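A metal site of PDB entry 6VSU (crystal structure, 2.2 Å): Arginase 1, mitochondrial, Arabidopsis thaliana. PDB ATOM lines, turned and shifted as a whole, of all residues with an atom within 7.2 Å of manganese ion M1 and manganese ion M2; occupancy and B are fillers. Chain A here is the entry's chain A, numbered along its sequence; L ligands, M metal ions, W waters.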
ATOM      1  N   ASP A 139      -8.005 -34.714  31.930  1.00  0.00           N
ATOM      2  CA  ASP A 139      -9.312 -34.057  32.145  1.00  0.00           C
ATOM      3  C   ASP A 139      -9.102 -32.542  32.243  1.00  0.00           C
ATOM      4  O   ASP A 139      -7.964 -32.095  32.323  1.00  0.00           O
ATOM      5  CB  ASP A 139     -10.044 -34.649  33.342  1.00  0.00           C
ATOM      6  CG  ASP A 139      -9.464 -34.360  34.714  1.00  0.00           C
ATOM      7  OD1 ASP A 139      -9.137 -33.187  34.987  1.00  0.00           O
ATOM      8  OD2 ASP A 139      -9.407 -35.320  35.511  1.00  0.00           O
ATOM      9  N   HIS A 140     -10.184 -31.791  32.337  1.00  0.00           N
ATOM     10  CA  HIS A 140     -10.148 -30.328  32.185  1.00  0.00           C
ATOM     11  C   HIS A 140      -9.560 -29.677  33.440  1.00  0.00           C
ATOM     12  O   HIS A 140      -9.207 -28.492  33.351  1.00  0.00           O
ATOM     13  CB  HIS A 140     -11.535 -29.789  31.810  1.00  0.00           C
ATOM     14  CG  HIS A 140     -11.446 -28.653  30.853  1.00  0.00           C
ATOM     15  ND1 HIS A 140     -12.398 -28.438  29.901  1.00  0.00           N
ATOM     16  CD2 HIS A 140     -10.466 -27.736  30.667  1.00  0.00           C
ATOM     17  CE1 HIS A 140     -12.054 -27.408  29.168  1.00  0.00           C
ATOM     18  NE2 HIS A 140     -10.843 -26.950  29.613  1.00  0.00           N
ATOM     19  N   SER A 141      -9.409 -30.396  34.569  1.00  0.00           N
ATOM     20  CA  SER A 141      -8.792 -29.796  35.782  1.00  0.00           C
ATOM     21  C   SER A 141      -7.401 -29.273  35.417  1.00  0.00           C
ATOM     22  O   SER A 141      -6.970 -28.296  36.038  1.00  0.00           O
ATOM     23  CB  SER A 141      -8.772 -30.746  36.941  1.00  0.00           C
ATOM     24  OG  SER A 141      -8.021 -31.925  36.648  1.00  0.00           O
ATOM     25  N   HIS A 162     -12.168 -20.516  25.247  1.00  0.00           N
ATOM     26  CA  HIS A 162     -12.471 -21.780  25.949  1.00  0.00           C
ATOM     27  C   HIS A 162     -13.532 -22.483  25.138  1.00  0.00           C
ATOM     28  O   HIS A 162     -14.682 -22.039  25.230  1.00  0.00           O
ATOM     29  CB  HIS A 162     -12.872 -21.464  27.406  1.00  0.00           C
ATOM     30  CG  HIS A 162     -13.426 -22.643  28.130  1.00  0.00           C
ATOM     31  ND1 HIS A 162     -14.324 -22.492  29.177  1.00  0.00           N
ATOM     32  CD2 HIS A 162     -13.233 -23.958  27.954  1.00  0.00           C
ATOM     33  CE1 HIS A 162     -14.661 -23.707  29.600  1.00  0.00           C
ATOM     34  NE2 HIS A 162     -14.012 -24.615  28.865  1.00  0.00           N
ATOM     35  N   LEU A 163     -13.170 -23.508  24.366  1.00  0.00           N
ATOM     36  CA  LEU A 163     -14.144 -24.306  23.575  1.00  0.00           C
ATOM     37  C   LEU A 163     -14.607 -25.539  24.373  1.00  0.00           C
ATOM     38  O   LEU A 163     -13.792 -26.431  24.694  1.00  0.00           O
ATOM     39  CB  LEU A 163     -13.454 -24.699  22.267  1.00  0.00           C
ATOM     40  CG  LEU A 163     -13.172 -23.546  21.288  1.00  0.00           C
ATOM     41  CD1 LEU A 163     -12.097 -23.915  20.285  1.00  0.00           C
ATOM     42  CD2 LEU A 163     -14.423 -23.195  20.556  1.00  0.00           C
ATOM     43  N   ASP A 164     -15.913 -25.627  24.674  1.00  0.00           N
ATOM     44  CA  ASP A 164     -16.439 -26.681  25.565  1.00  0.00           C
ATOM     45  C   ASP A 164     -17.966 -26.695  25.504  1.00  0.00           C
ATOM     46  O   ASP A 164     -18.565 -25.622  25.353  1.00  0.00           O
ATOM     47  CB  ASP A 164     -15.925 -26.394  26.966  1.00  0.00           C
ATOM     48  CG  ASP A 164     -15.894 -27.583  27.908  1.00  0.00           C
ATOM     49  OD1 ASP A 164     -16.770 -28.467  27.794  1.00  0.00           O
ATOM     50  OD2 ASP A 164     -14.967 -27.627  28.733  1.00  0.00           O
ATOM     51  N   ALA A 165     -18.583 -27.878  25.569  1.00  0.00           N
ATOM     52  CA  ALA A 165     -20.024 -28.021  25.846  1.00  0.00           C
ATOM     53  C   ALA A 165     -20.380 -27.398  27.198  1.00  0.00           C
ATOM     54  O   ALA A 165     -21.552 -26.954  27.364  1.00  0.00           O
ATOM     55  CB  ALA A 165     -20.453 -29.447  25.821  1.00  0.00           C
ATOM     56  N   HIS A 166     -19.422 -27.407  28.132  1.00  0.00           N
ATOM     57  CA  HIS A 166     -19.659 -27.065  29.562  1.00  0.00           C
ATOM     58  C   HIS A 166     -18.820 -25.845  29.956  1.00  0.00           C
ATOM     59  O   HIS A 166     -17.702 -25.664  29.482  1.00  0.00           O
ATOM     60  CB  HIS A 166     -19.279 -28.287  30.445  1.00  0.00           C
ATOM     61  CG  HIS A 166     -19.835 -29.602  29.959  1.00  0.00           C
ATOM     62  ND1 HIS A 166     -19.131 -30.394  29.096  1.00  0.00           N
ATOM     63  CD2 HIS A 166     -21.013 -30.240  30.236  1.00  0.00           C
ATOM     64  CE1 HIS A 166     -19.876 -31.464  28.834  1.00  0.00           C
ATOM     65  NE2 HIS A 166     -21.027 -31.394  29.541  1.00  0.00           N
ATOM     66  N   PRO A 167     -19.298 -24.991  30.895  1.00  0.00           N
ATOM     67  CA  PRO A 167     -18.508 -23.826  31.283  1.00  0.00           C
ATOM     68  C   PRO A 167     -17.397 -24.108  32.324  1.00  0.00           C
ATOM     69  O   PRO A 167     -16.490 -23.295  32.426  1.00  0.00           O
ATOM     70  CB  PRO A 167     -19.569 -22.835  31.766  1.00  0.00           C
ATOM     71  CG  PRO A 167     -20.733 -23.683  32.228  1.00  0.00           C
ATOM     72  CD  PRO A 167     -20.629 -25.012  31.515  1.00  0.00           C
ATOM     73  N   ASP A 168     -17.473 -25.235  33.046  1.00  0.00           N
ATOM     74  CA  ASP A 168     -16.432 -25.700  34.005  1.00  0.00           C
ATOM     75  C   ASP A 168     -16.140 -24.576  35.012  1.00  0.00           C
ATOM     76  O   ASP A 168     -14.980 -24.258  35.301  1.00  0.00           O
ATOM     77  CB  ASP A 168     -15.186 -26.200  33.262  1.00  0.00           C
ATOM     78  CG  ASP A 168     -15.459 -27.446  32.433  1.00  0.00           C
ATOM     79  OD1 ASP A 168     -16.522 -28.072  32.628  1.00  0.00           O
ATOM     80  OD2 ASP A 168     -14.567 -27.801  31.620  1.00  0.00           O
ATOM     81  N   HIS A 180     -12.715 -31.168  37.402  1.00  0.00           N
ATOM     82  CA  HIS A 180     -12.641 -30.747  35.980  1.00  0.00           C
ATOM     83  C   HIS A 180     -13.786 -29.766  35.647  1.00  0.00           C
ATOM     84  O   HIS A 180     -13.754 -29.164  34.558  1.00  0.00           O
ATOM     85  CB  HIS A 180     -12.659 -31.981  35.065  1.00  0.00           C
ATOM     86  CG  HIS A 180     -13.930 -32.751  34.973  1.00  0.00           C
ATOM     87  ND1 HIS A 180     -14.158 -33.621  33.910  1.00  0.00           N
ATOM     88  CD2 HIS A 180     -15.013 -32.850  35.756  1.00  0.00           C
ATOM     89  CE1 HIS A 180     -15.343 -34.202  34.048  1.00  0.00           C
ATOM     90  NE2 HIS A 180     -15.892 -33.738  35.149  1.00  0.00           N
ATOM     91  N   ALA A 181     -14.799 -29.669  36.515  1.00  0.00           N
ATOM     92  CA  ALA A 181     -15.970 -28.813  36.315  1.00  0.00           C
ATOM     93  C   ALA A 181     -15.777 -27.507  37.076  1.00  0.00           C
ATOM     94  O   ALA A 181     -16.754 -26.790  37.132  1.00  0.00           O
ATOM     95  CB  ALA A 181     -17.219 -29.525  36.764  1.00  0.00           C
ATOM     96  N   SER A 183     -12.365 -25.805  36.829  1.00  0.00           N
ATOM     97  CA  SER A 183     -11.046 -25.291  36.375  1.00  0.00           C
ATOM     98  C   SER A 183     -11.135 -23.780  36.120  1.00  0.00           C
ATOM     99  O   SER A 183     -10.204 -23.072  36.425  1.00  0.00           O
ATOM    100  CB  SER A 183     -10.509 -25.993  35.131  1.00  0.00           C
ATOM    101  OG  SER A 183     -10.899 -27.343  35.112  1.00  0.00           O
ATOM    102  N   PHE A 184     -12.250 -23.335  35.540  1.00  0.00           N
ATOM    103  CA  PHE A 184     -12.427 -21.942  35.061  1.00  0.00           C
ATOM    104  C   PHE A 184     -12.827 -21.029  36.230  1.00  0.00           C
ATOM    105  O   PHE A 184     -12.433 -19.878  36.190  1.00  0.00           O
ATOM    106  CB  PHE A 184     -13.293 -21.939  33.803  1.00  0.00           C
ATOM    107  CG  PHE A 184     -12.496 -22.459  32.641  1.00  0.00           C
ATOM    108  CD1 PHE A 184     -11.605 -21.636  31.961  1.00  0.00           C
ATOM    109  CD2 PHE A 184     -12.517 -23.801  32.317  1.00  0.00           C
ATOM    110  CE1 PHE A 184     -10.814 -22.134  30.939  1.00  0.00           C
ATOM    111  CE2 PHE A 184     -11.748 -24.296  31.286  1.00  0.00           C
ATOM    112  CZ  PHE A 184     -10.891 -23.462  30.594  1.00  0.00           C
ATOM    113  N   SER A 247      -8.056 -23.079  25.335  1.00  0.00           N
ATOM    114  CA  SER A 247      -8.392 -24.402  25.937  1.00  0.00           C
ATOM    115  C   SER A 247      -9.443 -25.102  25.072  1.00  0.00           C
ATOM    116  O   SER A 247     -10.493 -24.511  24.833  1.00  0.00           O
ATOM    117  CB  SER A 247      -8.864 -24.269  27.349  1.00  0.00           C
ATOM    118  OG  SER A 247      -9.226 -25.548  27.845  1.00  0.00           O
ATOM    119  N   ILE A 248      -9.203 -26.325  24.634  1.00  0.00           N
ATOM    120  CA  ILE A 248     -10.217 -27.033  23.803  1.00  0.00           C
ATOM    121  C   ILE A 248     -10.624 -28.338  24.479  1.00  0.00           C
ATOM    122  O   ILE A 248      -9.775 -29.233  24.584  1.00  0.00           O
ATOM    123  CB  ILE A 248      -9.704 -27.296  22.385  1.00  0.00           C
ATOM    124  CG1 ILE A 248      -9.201 -25.990  21.757  1.00  0.00           C
ATOM    125  CG2 ILE A 248     -10.809 -27.966  21.560  1.00  0.00           C
ATOM    126  CD1 ILE A 248      -8.726 -26.176  20.356  1.00  0.00           C
ATOM    127  N   ASP A 249     -11.850 -28.385  24.955  1.00  0.00           N
ATOM    128  CA  ASP A 249     -12.538 -29.632  25.399  1.00  0.00           C
ATOM    129  C   ASP A 249     -13.095 -30.264  24.116  1.00  0.00           C
ATOM    130  O   ASP A 249     -13.963 -29.645  23.431  1.00  0.00           O
ATOM    131  CB  ASP A 249     -13.629 -29.338  26.420  1.00  0.00           C
ATOM    132  CG  ASP A 249     -14.307 -30.572  27.017  1.00  0.00           C
ATOM    133  OD1 ASP A 249     -14.383 -31.616  26.289  1.00  0.00           O
ATOM    134  OD2 ASP A 249     -14.800 -30.437  28.166  1.00  0.00           O
ATOM    135  N   VAL A 250     -12.572 -31.412  23.781  1.00  0.00           N
ATOM    136  CA  VAL A 250     -13.046 -32.201  22.615  1.00  0.00           C
ATOM    137  C   VAL A 250     -14.600 -32.273  22.594  1.00  0.00           C
ATOM    138  O   VAL A 250     -15.160 -32.258  21.470  1.00  0.00           O
ATOM    139  CB  VAL A 250     -12.335 -33.557  22.680  1.00  0.00           C
ATOM    140  CG1 VAL A 250     -12.976 -34.602  21.792  1.00  0.00           C
ATOM    141  CG2 VAL A 250     -10.880 -33.370  22.284  1.00  0.00           C
ATOM    142  N   ASP A 251     -15.289 -32.229  23.738  1.00  0.00           N
ATOM    143  CA  ASP A 251     -16.789 -32.253  23.718  1.00  0.00           C
ATOM    144  C   ASP A 251     -17.374 -30.906  23.234  1.00  0.00           C
ATOM    145  O   ASP A 251     -18.651 -30.763  23.231  1.00  0.00           O
ATOM    146  CB  ASP A 251     -17.377 -32.721  25.057  1.00  0.00           C
ATOM    147  CG  ASP A 251     -17.258 -31.755  26.210  1.00  0.00           C
ATOM    148  OD1 ASP A 251     -17.196 -30.520  25.965  1.00  0.00           O
ATOM    149  OD2 ASP A 251     -17.150 -32.264  27.376  1.00  0.00           O
ATOM    150  N   CYS A 252     -16.545 -29.945  22.781  1.00  0.00           N
ATOM    151  CA  CYS A 252     -17.075 -28.753  22.082  1.00  0.00           C
ATOM    152  C   CYS A 252     -17.725 -29.204  20.779  1.00  0.00           C
ATOM    153  O   CYS A 252     -18.691 -28.542  20.346  1.00  0.00           O
ATOM    154  CB  CYS A 252     -16.052 -27.646  21.841  1.00  0.00           C
ATOM    155  SG  CYS A 252     -14.781 -28.038  20.612  1.00  0.00           S
ATOM    156  N   HIS A 263     -18.586 -36.990  28.440  1.00  0.00           N
ATOM    157  CA  HIS A 263     -19.904 -36.307  28.452  1.00  0.00           C
ATOM    158  C   HIS A 263     -20.476 -36.142  27.044  1.00  0.00           C
ATOM    159  O   HIS A 263     -20.208 -35.122  26.417  1.00  0.00           O
ATOM    160  CB  HIS A 263     -19.721 -34.992  29.172  1.00  0.00           C
ATOM    161  CG  HIS A 263     -19.210 -35.235  30.553  1.00  0.00           C
ATOM    162  ND1 HIS A 263     -20.045 -35.388  31.625  1.00  0.00           N
ATOM    163  CD2 HIS A 263     -17.939 -35.380  31.006  1.00  0.00           C
ATOM    164  CE1 HIS A 263     -19.316 -35.645  32.696  1.00  0.00           C
ATOM    165  NE2 HIS A 263     -18.002 -35.662  32.343  1.00  0.00           N
ATOM    166  N   VAL A 291      -8.064 -31.287  25.703  1.00  0.00           N
ATOM    167  CA  VAL A 291      -8.339 -32.067  26.942  1.00  0.00           C
ATOM    168  C   VAL A 291      -9.615 -32.861  26.716  1.00  0.00           C
ATOM    169  O   VAL A 291     -10.314 -32.597  25.748  1.00  0.00           O
ATOM    170  CB  VAL A 291      -8.472 -31.172  28.178  1.00  0.00           C
ATOM    171  CG1 VAL A 291      -7.269 -30.269  28.379  1.00  0.00           C
ATOM    172  CG2 VAL A 291      -9.738 -30.340  28.118  1.00  0.00           C
ATOM    173  N   GLU A 292      -9.858 -33.824  27.593  1.00  0.00           N
ATOM    174  CA  GLU A 292     -11.128 -34.593  27.718  1.00  0.00           C
ATOM    175  C   GLU A 292     -11.367 -35.543  26.548  1.00  0.00           C
ATOM    176  O   GLU A 292     -12.486 -36.023  26.414  1.00  0.00           O
ATOM    177  CB  GLU A 292     -12.321 -33.667  27.897  1.00  0.00           C
ATOM    178  CG  GLU A 292     -12.326 -32.998  29.230  1.00  0.00           C
ATOM    179  CD  GLU A 292     -12.604 -33.833  30.459  1.00  0.00           C
ATOM    180  OE1 GLU A 292     -12.978 -35.012  30.299  1.00  0.00           O
ATOM    181  OE2 GLU A 292     -12.425 -33.277  31.591  1.00  0.00           O
HETATM  182  N1  LIG L   1     -22.388 -32.990  34.812  1.00  0.00           N
HETATM  183  C1  LIG L   1     -21.312 -31.943  34.825  1.00  0.00           C
HETATM  184  C2  LIG L   1     -20.310 -32.188  33.678  1.00  0.00           C
HETATM  185  C3  LIG L   1     -18.986 -31.464  33.810  1.00  0.00           C
HETATM  186  C4  LIG L   1     -18.039 -31.756  32.664  1.00  0.00           C
HETATM  187  N2  LIG L   1     -16.683 -31.202  32.774  1.00  0.00           N
HETATM  188  C5  LIG L   1     -21.971 -30.560  34.684  1.00  0.00           C
HETATM  189  O1  LIG L   1     -21.419 -29.669  34.029  1.00  0.00           O
HETATM  190  O2  LIG L   1     -23.062 -30.299  35.216  1.00  0.00           O
HETATM  191 MN    MN M   1     -14.611 -28.992  30.129  1.00  0.00          MN
HETATM  192 MN    MN M   2     -16.931 -30.407  28.412  1.00  0.00          MN
HETATM  193  O   HOH W   1     -15.923 -32.528  30.286  1.00  0.00           O
HETATM  194  O   HOH W   2     -16.664 -30.200  30.386  1.00  0.00           O
HETATM  195  O   HOH W   3     -14.504 -30.365  32.065  1.00  0.00           O
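Of the 23 residues printed, 4 come within 4 Å of manganese ion M2.
Along chain A the residues within 4 Å of manganese ion M2 span positions 164 to 251.
The nearest printed residue that does not touch manganese ion M2 is Ala 165 (4.1 Å).
Along chain A the residues within 4 Å of manganese ion M1 span positions 140 to 249.
OD1 of Asp 168 lies within salt-bridge range of N2 of the ligand.
Water W3 lies within hydrogen-bond range of a nitrogen (N2) of the ligand (2.4 Å), the backbone carbonyl oxygen of His 180 (2.9 Å) and the side-chain carboxylate of Asp 168 (3.1 Å).
Water W2 lies within hydrogen-bond range of a nitrogen (N2) of the ligand (2.6 Å) and the side-chain carboxylate of Asp 168 (3.1 Å).
The side-chain carboxylate (OD2) of Asp 168 binds manganese ion M1, at 1.9 Å.
OD2 of Asp 164 binds manganese ion M1 (2.0 Å).
ND1 of His 140 is bound to manganese ion M1.
Water W3 binds manganese ion M1, 2.4 Å away.
Manganese ion M1 is bound by water W2 (2.4 Å).
OD2 of Asp 249 is bound to manganese ion M1 (2.4 Å).
Manganese ion M1 has six donor atoms within binding distance.
The side-chain carboxylate of Asp 164 lies close to a ring nitrogen (NE2) of His 162 (3.2 Å).
NE2 of His 140 lies within hydrogen-bond range of OG of Ser 247.
O of Asp 168 is in hydrogen-bond range of N of Ser 183 (3.4 Å).
N of His 140 lies within hydrogen-bond range of OE2 of Glu 292 (2.8 Å).
The backbone carbonyl oxygen (O) of His 140 lies within hydrogen-bond range of the side-chain hydroxyl (OG) of Ser 183.
O of Asp 249 lies close to SG of Cys 252, 3.3 Å away.
The backbone carbonyl oxygen of Asp 168 sits at hydrogen-bond distance from the backbone NH of Phe 184, 2.9 Å away.
The backbone NH of Asp 249 sits at hydrogen-bond distance from the backbone carbonyl oxygen of Leu 163.
Manganese ion M2 is bound by water W2 (2.0 Å), the side-chain carboxylate (OD1) of Asp 164 (2.0 Å), the side-chain carboxylate (OD2) of Asp 251 (2.1 Å), the side-chain carboxylate (OD2) of Asp 249 (2.1 Å), a ring nitrogen (ND1) of His 166 (2.3 Å) and the side-chain carboxylate (OD1) of Asp 251 (2.5 Å).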
